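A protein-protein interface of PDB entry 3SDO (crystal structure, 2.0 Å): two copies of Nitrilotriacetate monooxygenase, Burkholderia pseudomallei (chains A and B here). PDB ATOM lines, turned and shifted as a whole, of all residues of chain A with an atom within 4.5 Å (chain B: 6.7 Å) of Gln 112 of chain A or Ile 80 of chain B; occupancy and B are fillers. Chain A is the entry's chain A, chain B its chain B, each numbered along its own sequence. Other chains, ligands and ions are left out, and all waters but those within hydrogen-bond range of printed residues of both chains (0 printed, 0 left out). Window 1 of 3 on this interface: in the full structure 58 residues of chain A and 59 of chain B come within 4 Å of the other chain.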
ATOM      1  N   ILE A  80       4.854 -23.672 -16.264  1.00  0.00           N
ATOM      2  CA  ILE A  80       5.564 -24.885 -15.815  1.00  0.00           C
ATOM      3  C   ILE A  80       7.053 -24.578 -15.656  1.00  0.00           C
ATOM      4  O   ILE A  80       7.648 -24.935 -14.630  1.00  0.00           O
ATOM      5  CB  ILE A  80       5.367 -26.075 -16.759  1.00  0.00           C
ATOM      6  CG1 ILE A  80       3.904 -26.502 -16.775  1.00  0.00           C
ATOM      7  CG2 ILE A  80       6.309 -27.265 -16.382  1.00  0.00           C
ATOM      8  CD1 ILE A  80       3.423 -27.114 -15.452  1.00  0.00           C
ATOM      9  N   SER A  81       7.650 -23.948 -16.673  1.00  0.00           N
ATOM     10  CA  SER A  81       9.043 -23.539 -16.601  1.00  0.00           C
ATOM     11  C   SER A  81       9.293 -22.588 -15.419  1.00  0.00           C
ATOM     12  O   SER A  81      10.219 -22.795 -14.636  1.00  0.00           O
ATOM     13  CB  SER A  81       9.532 -22.881 -17.902  1.00  0.00           C
ATOM     14  OG  SER A  81       8.701 -21.806 -18.325  1.00  0.00           O
ATOM     15  N   MET A  99      -3.180 -23.605 -16.502  1.00  0.00           N
ATOM     16  CA  MET A  99      -3.069 -24.270 -17.787  1.00  0.00           C
ATOM     17  C   MET A  99      -4.463 -24.622 -18.298  1.00  0.00           C
ATOM     18  O   MET A  99      -5.320 -25.050 -17.539  1.00  0.00           O
ATOM     19  CB  MET A  99      -2.193 -25.517 -17.721  1.00  0.00           C
ATOM     20  CG  MET A  99      -1.725 -25.960 -19.105  1.00  0.00           C
ATOM     21  SD  MET A  99      -0.627 -27.366 -19.010  1.00  0.00           S
ATOM     22  CE  MET A  99       0.883 -26.616 -18.382  1.00  0.00           C
ATOM     23  N   ASN A 108       0.191 -34.751 -21.298  1.00  0.00           N
ATOM     24  CA  ASN A 108       1.257 -33.770 -21.086  1.00  0.00           C
ATOM     25  C   ASN A 108       1.028 -32.938 -19.819  1.00  0.00           C
ATOM     26  O   ASN A 108       1.968 -32.647 -19.091  1.00  0.00           O
ATOM     27  CB  ASN A 108       1.396 -32.818 -22.301  1.00  0.00           C
ATOM     28  CG  ASN A 108       1.947 -33.516 -23.534  1.00  0.00           C
ATOM     29  OD1 ASN A 108       2.682 -34.499 -23.416  1.00  0.00           O
ATOM     30  ND2 ASN A 108       1.589 -33.019 -24.727  1.00  0.00           N
ATOM     31  N   VAL A 109      -0.212 -32.510 -19.593  1.00  0.00           N
ATOM     32  CA  VAL A 109      -0.554 -31.781 -18.378  1.00  0.00           C
ATOM     33  C   VAL A 109      -0.233 -32.610 -17.149  1.00  0.00           C
ATOM     34  O   VAL A 109       0.416 -32.139 -16.207  1.00  0.00           O
ATOM     35  CB  VAL A 109      -2.043 -31.357 -18.383  1.00  0.00           C
ATOM     36  CG1 VAL A 109      -2.446 -30.741 -17.011  1.00  0.00           C
ATOM     37  CG2 VAL A 109      -2.286 -30.353 -19.537  1.00  0.00           C
ATOM     38  N   ALA A 110      -0.673 -33.853 -17.161  1.00  0.00           N
ATOM     39  CA  ALA A 110      -0.419 -34.743 -16.045  1.00  0.00           C
ATOM     40  C   ALA A 110       1.088 -34.874 -15.747  1.00  0.00           C
ATOM     41  O   ALA A 110       1.508 -34.754 -14.575  1.00  0.00           O
ATOM     42  CB  ALA A 110      -1.074 -36.105 -16.302  1.00  0.00           C
ATOM     43  N   ARG A 111       1.894 -35.078 -16.786  1.00  0.00           N
ATOM     44  CA  ARG A 111       3.343 -35.246 -16.621  1.00  0.00           C
ATOM     45  C   ARG A 111       4.013 -33.981 -16.138  1.00  0.00           C
ATOM     46  O   ARG A 111       4.855 -34.036 -15.250  1.00  0.00           O
ATOM     47  CB  ARG A 111       4.027 -35.652 -17.938  1.00  0.00           C
ATOM     48  CG  ARG A 111       3.762 -37.071 -18.431  1.00  0.00           C
ATOM     49  CD  ARG A 111       4.672 -37.400 -19.599  1.00  0.00           C
ATOM     50  NE  ARG A 111       6.069 -37.530 -19.191  1.00  0.00           N
ATOM     51  CZ  ARG A 111       7.123 -37.250 -19.954  1.00  0.00           C
ATOM     52  NH1 ARG A 111       6.981 -36.767 -21.182  1.00  0.00           N
ATOM     53  NH2 ARG A 111       8.339 -37.429 -19.464  1.00  0.00           N
ATOM     54  N   GLN A 112       3.648 -32.841 -16.714  1.00  0.00           N
ATOM     55  CA  GLN A 112       4.348 -31.610 -16.404  1.00  0.00           C
ATOM     56  C   GLN A 112       4.030 -31.166 -14.999  1.00  0.00           C
ATOM     57  O   GLN A 112       4.950 -30.852 -14.244  1.00  0.00           O
ATOM     58  CB  GLN A 112       4.082 -30.507 -17.447  1.00  0.00           C
ATOM     59  CG  GLN A 112       4.691 -30.826 -18.798  1.00  0.00           C
ATOM     60  CD  GLN A 112       4.665 -29.661 -19.764  1.00  0.00           C
ATOM     61  OE1 GLN A 112       3.704 -28.903 -19.814  1.00  0.00           O
ATOM     62  NE2 GLN A 112       5.732 -29.512 -20.542  1.00  0.00           N
ATOM     63  N   PHE A 113       2.754 -31.196 -14.612  1.00  0.00           N
ATOM     64  CA  PHE A 113       2.387 -30.921 -13.216  1.00  0.00           C
ATOM     65  C   PHE A 113       2.889 -31.974 -12.198  1.00  0.00           C
ATOM     66  O   PHE A 113       3.305 -31.595 -11.098  1.00  0.00           O
ATOM     67  CB  PHE A 113       0.874 -30.676 -13.051  1.00  0.00           C
ATOM     68  CG  PHE A 113       0.455 -29.292 -13.419  1.00  0.00           C
ATOM     69  CD1 PHE A 113       0.740 -28.217 -12.581  1.00  0.00           C
ATOM     70  CD2 PHE A 113      -0.193 -29.040 -14.605  1.00  0.00           C
ATOM     71  CE1 PHE A 113       0.352 -26.939 -12.917  1.00  0.00           C
ATOM     72  CE2 PHE A 113      -0.559 -27.742 -14.937  1.00  0.00           C
ATOM     73  CZ  PHE A 113      -0.261 -26.697 -14.073  1.00  0.00           C
ATOM     74  N   ALA A 114       2.869 -33.263 -12.553  1.00  0.00           N
ATOM     75  CA  ALA A 114       3.422 -34.322 -11.657  1.00  0.00           C
ATOM     76  C   ALA A 114       4.933 -34.155 -11.418  1.00  0.00           C
ATOM     77  O   ALA A 114       5.429 -34.408 -10.318  1.00  0.00           O
ATOM     78  CB  ALA A 114       3.133 -35.707 -12.193  1.00  0.00           C
ATOM     79  N   SER A 115       5.636 -33.684 -12.441  1.00  0.00           N
ATOM     80  CA  SER A 115       7.079 -33.498 -12.374  1.00  0.00           C
ATOM     81  C   SER A 115       7.394 -32.278 -11.509  1.00  0.00           C
ATOM     82  O   SER A 115       8.270 -32.334 -10.644  1.00  0.00           O
ATOM     83  CB  SER A 115       7.667 -33.418 -13.797  1.00  0.00           C
ATOM     84  OG  SER A 115       9.075 -33.258 -13.833  1.00  0.00           O
ATOM     85  N   LEU A 116       6.676 -31.178 -11.725  1.00  0.00           N
ATOM     86  CA  LEU A 116       6.782 -30.026 -10.820  1.00  0.00           C
ATOM     87  C   LEU A 116       6.499 -30.443  -9.370  1.00  0.00           C
ATOM     88  O   LEU A 116       7.243 -30.071  -8.447  1.00  0.00           O
ATOM     89  CB  LEU A 116       5.834 -28.897 -11.265  1.00  0.00           C
ATOM     90  CG  LEU A 116       5.608 -27.703 -10.329  1.00  0.00           C
ATOM     91  CD1 LEU A 116       6.928 -26.886 -10.186  1.00  0.00           C
ATOM     92  CD2 LEU A 116       4.427 -26.826 -10.828  1.00  0.00           C
ATOM     93  N   ILE B  59      18.411 -34.252 -21.778  1.00  0.00           N
ATOM     94  CA  ILE B  59      17.324 -35.046 -21.204  1.00  0.00           C
ATOM     95  C   ILE B  59      16.485 -35.623 -22.354  1.00  0.00           C
ATOM     96  O   ILE B  59      15.711 -34.911 -23.011  1.00  0.00           O
ATOM     97  CB  ILE B  59      16.435 -34.198 -20.264  1.00  0.00           C
ATOM     98  CG1 ILE B  59      17.288 -33.536 -19.171  1.00  0.00           C
ATOM     99  CG2 ILE B  59      15.306 -35.079 -19.650  1.00  0.00           C
ATOM    100  CD1 ILE B  59      18.029 -34.524 -18.256  1.00  0.00           C
ATOM    101  N   GLU B  78       9.743 -35.039 -16.272  1.00  0.00           N
ATOM    102  CA  GLU B  78       9.384 -34.456 -17.563  1.00  0.00           C
ATOM    103  C   GLU B  78      10.426 -33.374 -17.905  1.00  0.00           C
ATOM    104  O   GLU B  78      10.923 -32.714 -16.998  1.00  0.00           O
ATOM    105  CB  GLU B  78       7.955 -33.910 -17.463  1.00  0.00           C
ATOM    106  CG  GLU B  78       7.407 -33.252 -18.692  1.00  0.00           C
ATOM    107  CD  GLU B  78       7.902 -31.851 -18.873  1.00  0.00           C
ATOM    108  OE1 GLU B  78       8.243 -31.217 -17.837  1.00  0.00           O
ATOM    109  OE2 GLU B  78       7.966 -31.392 -20.050  1.00  0.00           O
ATOM    110  N   PRO B  79      10.756 -33.170 -19.203  1.00  0.00           N
ATOM    111  CA  PRO B  79      11.940 -32.353 -19.494  1.00  0.00           C
ATOM    112  C   PRO B  79      11.869 -30.850 -19.271  1.00  0.00           C
ATOM    113  O   PRO B  79      12.861 -30.305 -18.781  1.00  0.00           O
ATOM    114  CB  PRO B  79      12.255 -32.662 -20.978  1.00  0.00           C
ATOM    115  CG  PRO B  79      11.665 -33.999 -21.191  1.00  0.00           C
ATOM    116  CD  PRO B  79      10.349 -33.918 -20.400  1.00  0.00           C
ATOM    117  N   ILE B  80      10.763 -30.184 -19.628  1.00  0.00           N
ATOM    118  CA  ILE B  80      10.647 -28.733 -19.393  1.00  0.00           C
ATOM    119  C   ILE B  80      10.804 -28.432 -17.908  1.00  0.00           C
ATOM    120  O   ILE B  80      11.595 -27.580 -17.527  1.00  0.00           O
ATOM    121  CB  ILE B  80       9.321 -28.144 -19.927  1.00  0.00           C
ATOM    122  CG1 ILE B  80       9.239 -28.258 -21.456  1.00  0.00           C
ATOM    123  CG2 ILE B  80       9.147 -26.660 -19.503  1.00  0.00           C
ATOM    124  CD1 ILE B  80      10.388 -27.551 -22.239  1.00  0.00           C
ATOM    125  N   SER B  81      10.096 -29.160 -17.052  1.00  0.00           N
ATOM    126  CA  SER B  81      10.164 -28.901 -15.612  1.00  0.00           C
ATOM    127  C   SER B  81      11.538 -29.209 -15.054  1.00  0.00           C
ATOM    128  O   SER B  81      12.126 -28.405 -14.341  1.00  0.00           O
ATOM    129  CB  SER B  81       9.084 -29.676 -14.860  1.00  0.00           C
ATOM    130  OG  SER B  81       9.121 -31.027 -15.180  1.00  0.00           O
ATOM    131  N   LEU B  82      12.102 -30.354 -15.432  1.00  0.00           N
ATOM    132  CA  LEU B  82      13.427 -30.719 -14.945  1.00  0.00           C
ATOM    133  C   LEU B  82      14.483 -29.714 -15.397  1.00  0.00           C
ATOM    134  O   LEU B  82      15.318 -29.269 -14.597  1.00  0.00           O
ATOM    135  CB  LEU B  82      13.807 -32.131 -15.432  1.00  0.00           C
ATOM    136  CG  LEU B  82      15.184 -32.615 -15.005  1.00  0.00           C
ATOM    137  CD1 LEU B  82      15.296 -32.665 -13.485  1.00  0.00           C
ATOM    138  CD2 LEU B  82      15.524 -33.975 -15.643  1.00  0.00           C
ATOM    139  N   LEU B  83      14.473 -29.369 -16.689  1.00  0.00           N
ATOM    140  CA  LEU B  83      15.500 -28.473 -17.218  1.00  0.00           C
ATOM    141  C   LEU B  83      15.413 -27.075 -16.624  1.00  0.00           C
ATOM    142  O   LEU B  83      16.432 -26.396 -16.395  1.00  0.00           O
ATOM    143  CB  LEU B  83      15.475 -28.450 -18.740  1.00  0.00           C
ATOM    144  CG  LEU B  83      15.989 -29.738 -19.430  1.00  0.00           C
ATOM    145  CD1 LEU B  83      15.694 -29.662 -20.907  1.00  0.00           C
ATOM    146  CD2 LEU B  83      17.496 -29.934 -19.206  1.00  0.00           C
ATOM    147  N   SER B  84      14.202 -26.639 -16.349  1.00  0.00           N
ATOM    148  CA  SER B  84      13.990 -25.301 -15.795  1.00  0.00           C
ATOM    149  C   SER B  84      14.503 -25.224 -14.344  1.00  0.00           C
ATOM    150  O   SER B  84      15.096 -24.229 -13.945  1.00  0.00           O
ATOM    151  CB  SER B  84      12.512 -24.934 -15.866  1.00  0.00           C
ATOM    152  OG  SER B  84      12.059 -24.771 -17.207  1.00  0.00           O
ATOM    153  N   ALA B  85      14.261 -26.283 -13.567  1.00  0.00           N
ATOM    154  CA  ALA B  85      14.858 -26.411 -12.218  1.00  0.00           C
ATOM    155  C   ALA B  85      16.396 -26.488 -12.238  1.00  0.00           C
ATOM    156  O   ALA B  85      17.094 -25.838 -11.435  1.00  0.00           O
ATOM    157  CB  ALA B  85      14.256 -27.636 -11.509  1.00  0.00           C
ATOM    158  N   GLY B  97      16.342 -30.627 -24.230  1.00  0.00           N
ATOM    159  CA  GLY B  97      15.250 -31.519 -23.878  1.00  0.00           C
ATOM    160  C   GLY B  97      14.515 -32.031 -25.081  1.00  0.00           C
ATOM    161  O   GLY B  97      14.302 -31.315 -26.060  1.00  0.00           O
ATOM    162  N   THR B  98      14.156 -33.299 -25.029  1.00  0.00           N
ATOM    163  CA  THR B  98      13.355 -33.921 -26.066  1.00  0.00           C
ATOM    164  C   THR B  98      11.885 -33.502 -25.908  1.00  0.00           C
ATOM    165  O   THR B  98      11.323 -33.494 -24.793  1.00  0.00           O
ATOM    166  CB  THR B  98      13.461 -35.456 -25.983  1.00  0.00           C
ATOM    167  OG1 THR B  98      14.770 -35.864 -26.381  1.00  0.00           O
ATOM    168  CG2 THR B  98      12.402 -36.154 -26.845  1.00  0.00           C
ATOM    169  N   MET B  99      11.271 -33.170 -27.031  1.00  0.00           N
ATOM    170  CA  MET B  99       9.833 -33.045 -27.119  1.00  0.00           C
ATOM    171  C   MET B  99       9.371 -33.437 -28.528  1.00  0.00           C
ATOM    172  O   MET B  99      10.000 -33.095 -29.557  1.00  0.00           O
ATOM    173  CB  MET B  99       9.381 -31.630 -26.758  1.00  0.00           C
ATOM    174  CG  MET B  99       7.869 -31.507 -26.557  1.00  0.00           C
ATOM    175  SD  MET B  99       7.417 -29.880 -25.937  1.00  0.00           S
ATOM    176  CE  MET B  99       8.087 -29.964 -24.283  1.00  0.00           C
ATOM    177  N   VAL B 109       4.997 -25.545 -27.358  1.00  0.00           N
ATOM    178  CA  VAL B 109       6.414 -25.879 -27.467  1.00  0.00           C
ATOM    179  C   VAL B 109       7.261 -24.610 -27.536  1.00  0.00           C
ATOM    180  O   VAL B 109       8.257 -24.477 -26.838  1.00  0.00           O
ATOM    181  CB  VAL B 109       6.695 -26.742 -28.707  1.00  0.00           C
ATOM    182  CG1 VAL B 109       8.194 -26.966 -28.876  1.00  0.00           C
ATOM    183  CG2 VAL B 109       5.948 -28.085 -28.622  1.00  0.00           C
ATOM    184  N   GLN B 112       7.195 -22.862 -24.000  1.00  0.00           N
ATOM    185  CA  GLN B 112       7.941 -23.598 -22.974  1.00  0.00           C
ATOM    186  C   GLN B 112       9.461 -23.547 -23.169  1.00  0.00           C
ATOM    187  O   GLN B 112      10.213 -23.250 -22.221  1.00  0.00           O
ATOM    188  CB  GLN B 112       7.388 -25.024 -22.835  1.00  0.00           C
ATOM    189  CG  GLN B 112       5.964 -25.003 -22.211  1.00  0.00           C
ATOM    190  CD  GLN B 112       5.473 -26.361 -21.755  1.00  0.00           C
ATOM    191  OE1 GLN B 112       5.802 -27.375 -22.352  1.00  0.00           O
ATOM    192  NE2 GLN B 112       4.651 -26.380 -20.704  1.00  0.00           N
ATOM    193  N   PHE B 113       9.928 -23.746 -24.396  1.00  0.00           N
ATOM    194  CA  PHE B 113      11.355 -23.649 -24.636  1.00  0.00           C
ATOM    195  C   PHE B 113      11.881 -22.221 -24.588  1.00  0.00           C
ATOM    196  O   PHE B 113      13.011 -22.005 -24.131  1.00  0.00           O
ATOM    197  CB  PHE B 113      11.748 -24.351 -25.933  1.00  0.00           C
ATOM    198  CG  PHE B 113      11.877 -25.838 -25.781  1.00  0.00           C
ATOM    199  CD1 PHE B 113      13.009 -26.393 -25.203  1.00  0.00           C
ATOM    200  CD2 PHE B 113      10.868 -26.686 -26.213  1.00  0.00           C
ATOM    201  CE1 PHE B 113      13.124 -27.775 -25.065  1.00  0.00           C
ATOM    202  CE2 PHE B 113      10.991 -28.073 -26.106  1.00  0.00           C
ATOM    203  CZ  PHE B 113      12.098 -28.612 -25.522  1.00  0.00           C
ATOM    204  N   LEU B 116      12.195 -21.405 -20.777  1.00  0.00           N
ATOM    205  CA  LEU B 116      13.454 -22.020 -20.372  1.00  0.00           C
ATOM    206  C   LEU B 116      14.648 -21.207 -20.869  1.00  0.00           C
ATOM    207  O   LEU B 116      15.592 -20.949 -20.105  1.00  0.00           O
ATOM    208  CB  LEU B 116      13.548 -23.463 -20.902  1.00  0.00           C
ATOM    209  CG  LEU B 116      14.843 -24.240 -20.647  1.00  0.00           C
ATOM    210  CD1 LEU B 116      15.074 -24.393 -19.147  1.00  0.00           C
ATOM    211  CD2 LEU B 116      14.789 -25.611 -21.372  1.00  0.00           C
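OE1 of Gln 112 of chain B sits at hydrogen-bond distance from NE2 of Gln 112 of chain A, 2.8 Å away.
OG of Ser 115 of chain A is in hydrogen-bond range of N of Glu 78 of chain B (3.1 Å).
The side-chain amide nitrogen of Gln 112 of chain A is in hydrogen-bond range of the side-chain carboxylate of Glu 78 of chain B (3.0 Å).
OG of Ser 81 of chain B lies within hydrogen-bond range of OG of Ser 115 of chain A (2.6 Å).
The side-chain hydroxyl of Ser 81 of chain B is in hydrogen-bond range of the side-chain carboxylate of Glu 78 of chain B, at 2.8 Å.
The backbone NH of Ile 80 of chain B is in hydrogen-bond range of the side-chain carboxylate of Glu 78 of chain B, 3.1 Å away.
The backbone carbonyl oxygen of Ile 80 of chain B lies within hydrogen-bond range of the side-chain hydroxyl of Ser 84 of chain B (2.9 Å).
Ile 80 of chain A touches Ser 81 of chain B (CG2 to CB, 3.98 Å).
OG of Ser 84 of chain B touches CB of Ser 81 of chain A, 3.2 Å away.
NH2 of Arg 111 of chain A touches CA of Glu 78 of chain B, at 3.7 Å.
Ile 80 of chain B touches Gln 112 of chain A.
Of the printed residues of chain B, Ser 81 of chain A touches Ser 84.
Ile 80 of chain B touches one residue of chain A.
Of the printed residues of chain A, Ser 81 of chain B touches Ile 80 and Ser 115.
Of the printed residues of chain A, Gln 112 of chain B touches Gln 112.
The nearest residue of chain B that does not touch Gln 112 of chain A is Ser 81 of chain B (4.3 Å).
The nearest printed residue of chain B that does not touch Ser 115 of chain A is Leu 82 of chain B (4.5 Å).
Of the 12 printed residues of chain A, 5 touch a printed residue of chain B.
Hydrophobic or aromatic side chains of chain A within 4 Å of the printed part of chain B: Ile 80.
Printed residues of chain B that touch a printed residue of chain A: Glu 78, Ile 80, Ser 81, Ser 84 and Gln 112.
Hydrophobic or aromatic side chains of chain B that line the printed part of chain A: Ile 80.
Ile 80 of chain A touches Ser 81 of chain B, but with the chains exchanged Ser 81 of chain A does not touch Ile 80 of chain B (4.1 Å).
Gln 112 of chain A touches Ile 80 of chain B, but with the chains exchanged Ile 80 of chain A does not touch Gln 112 of chain B (4.001 Å).
Gln 112 of chain A touches its own counterpart, Gln 112 of chain B.
Positions printed for both chains: 80, 81, 99, 109, 112, 113 and 116.
Of the 8 pairs that touch across the chains among the printed residues, 1 has its exchanged pair printed and touching as well.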
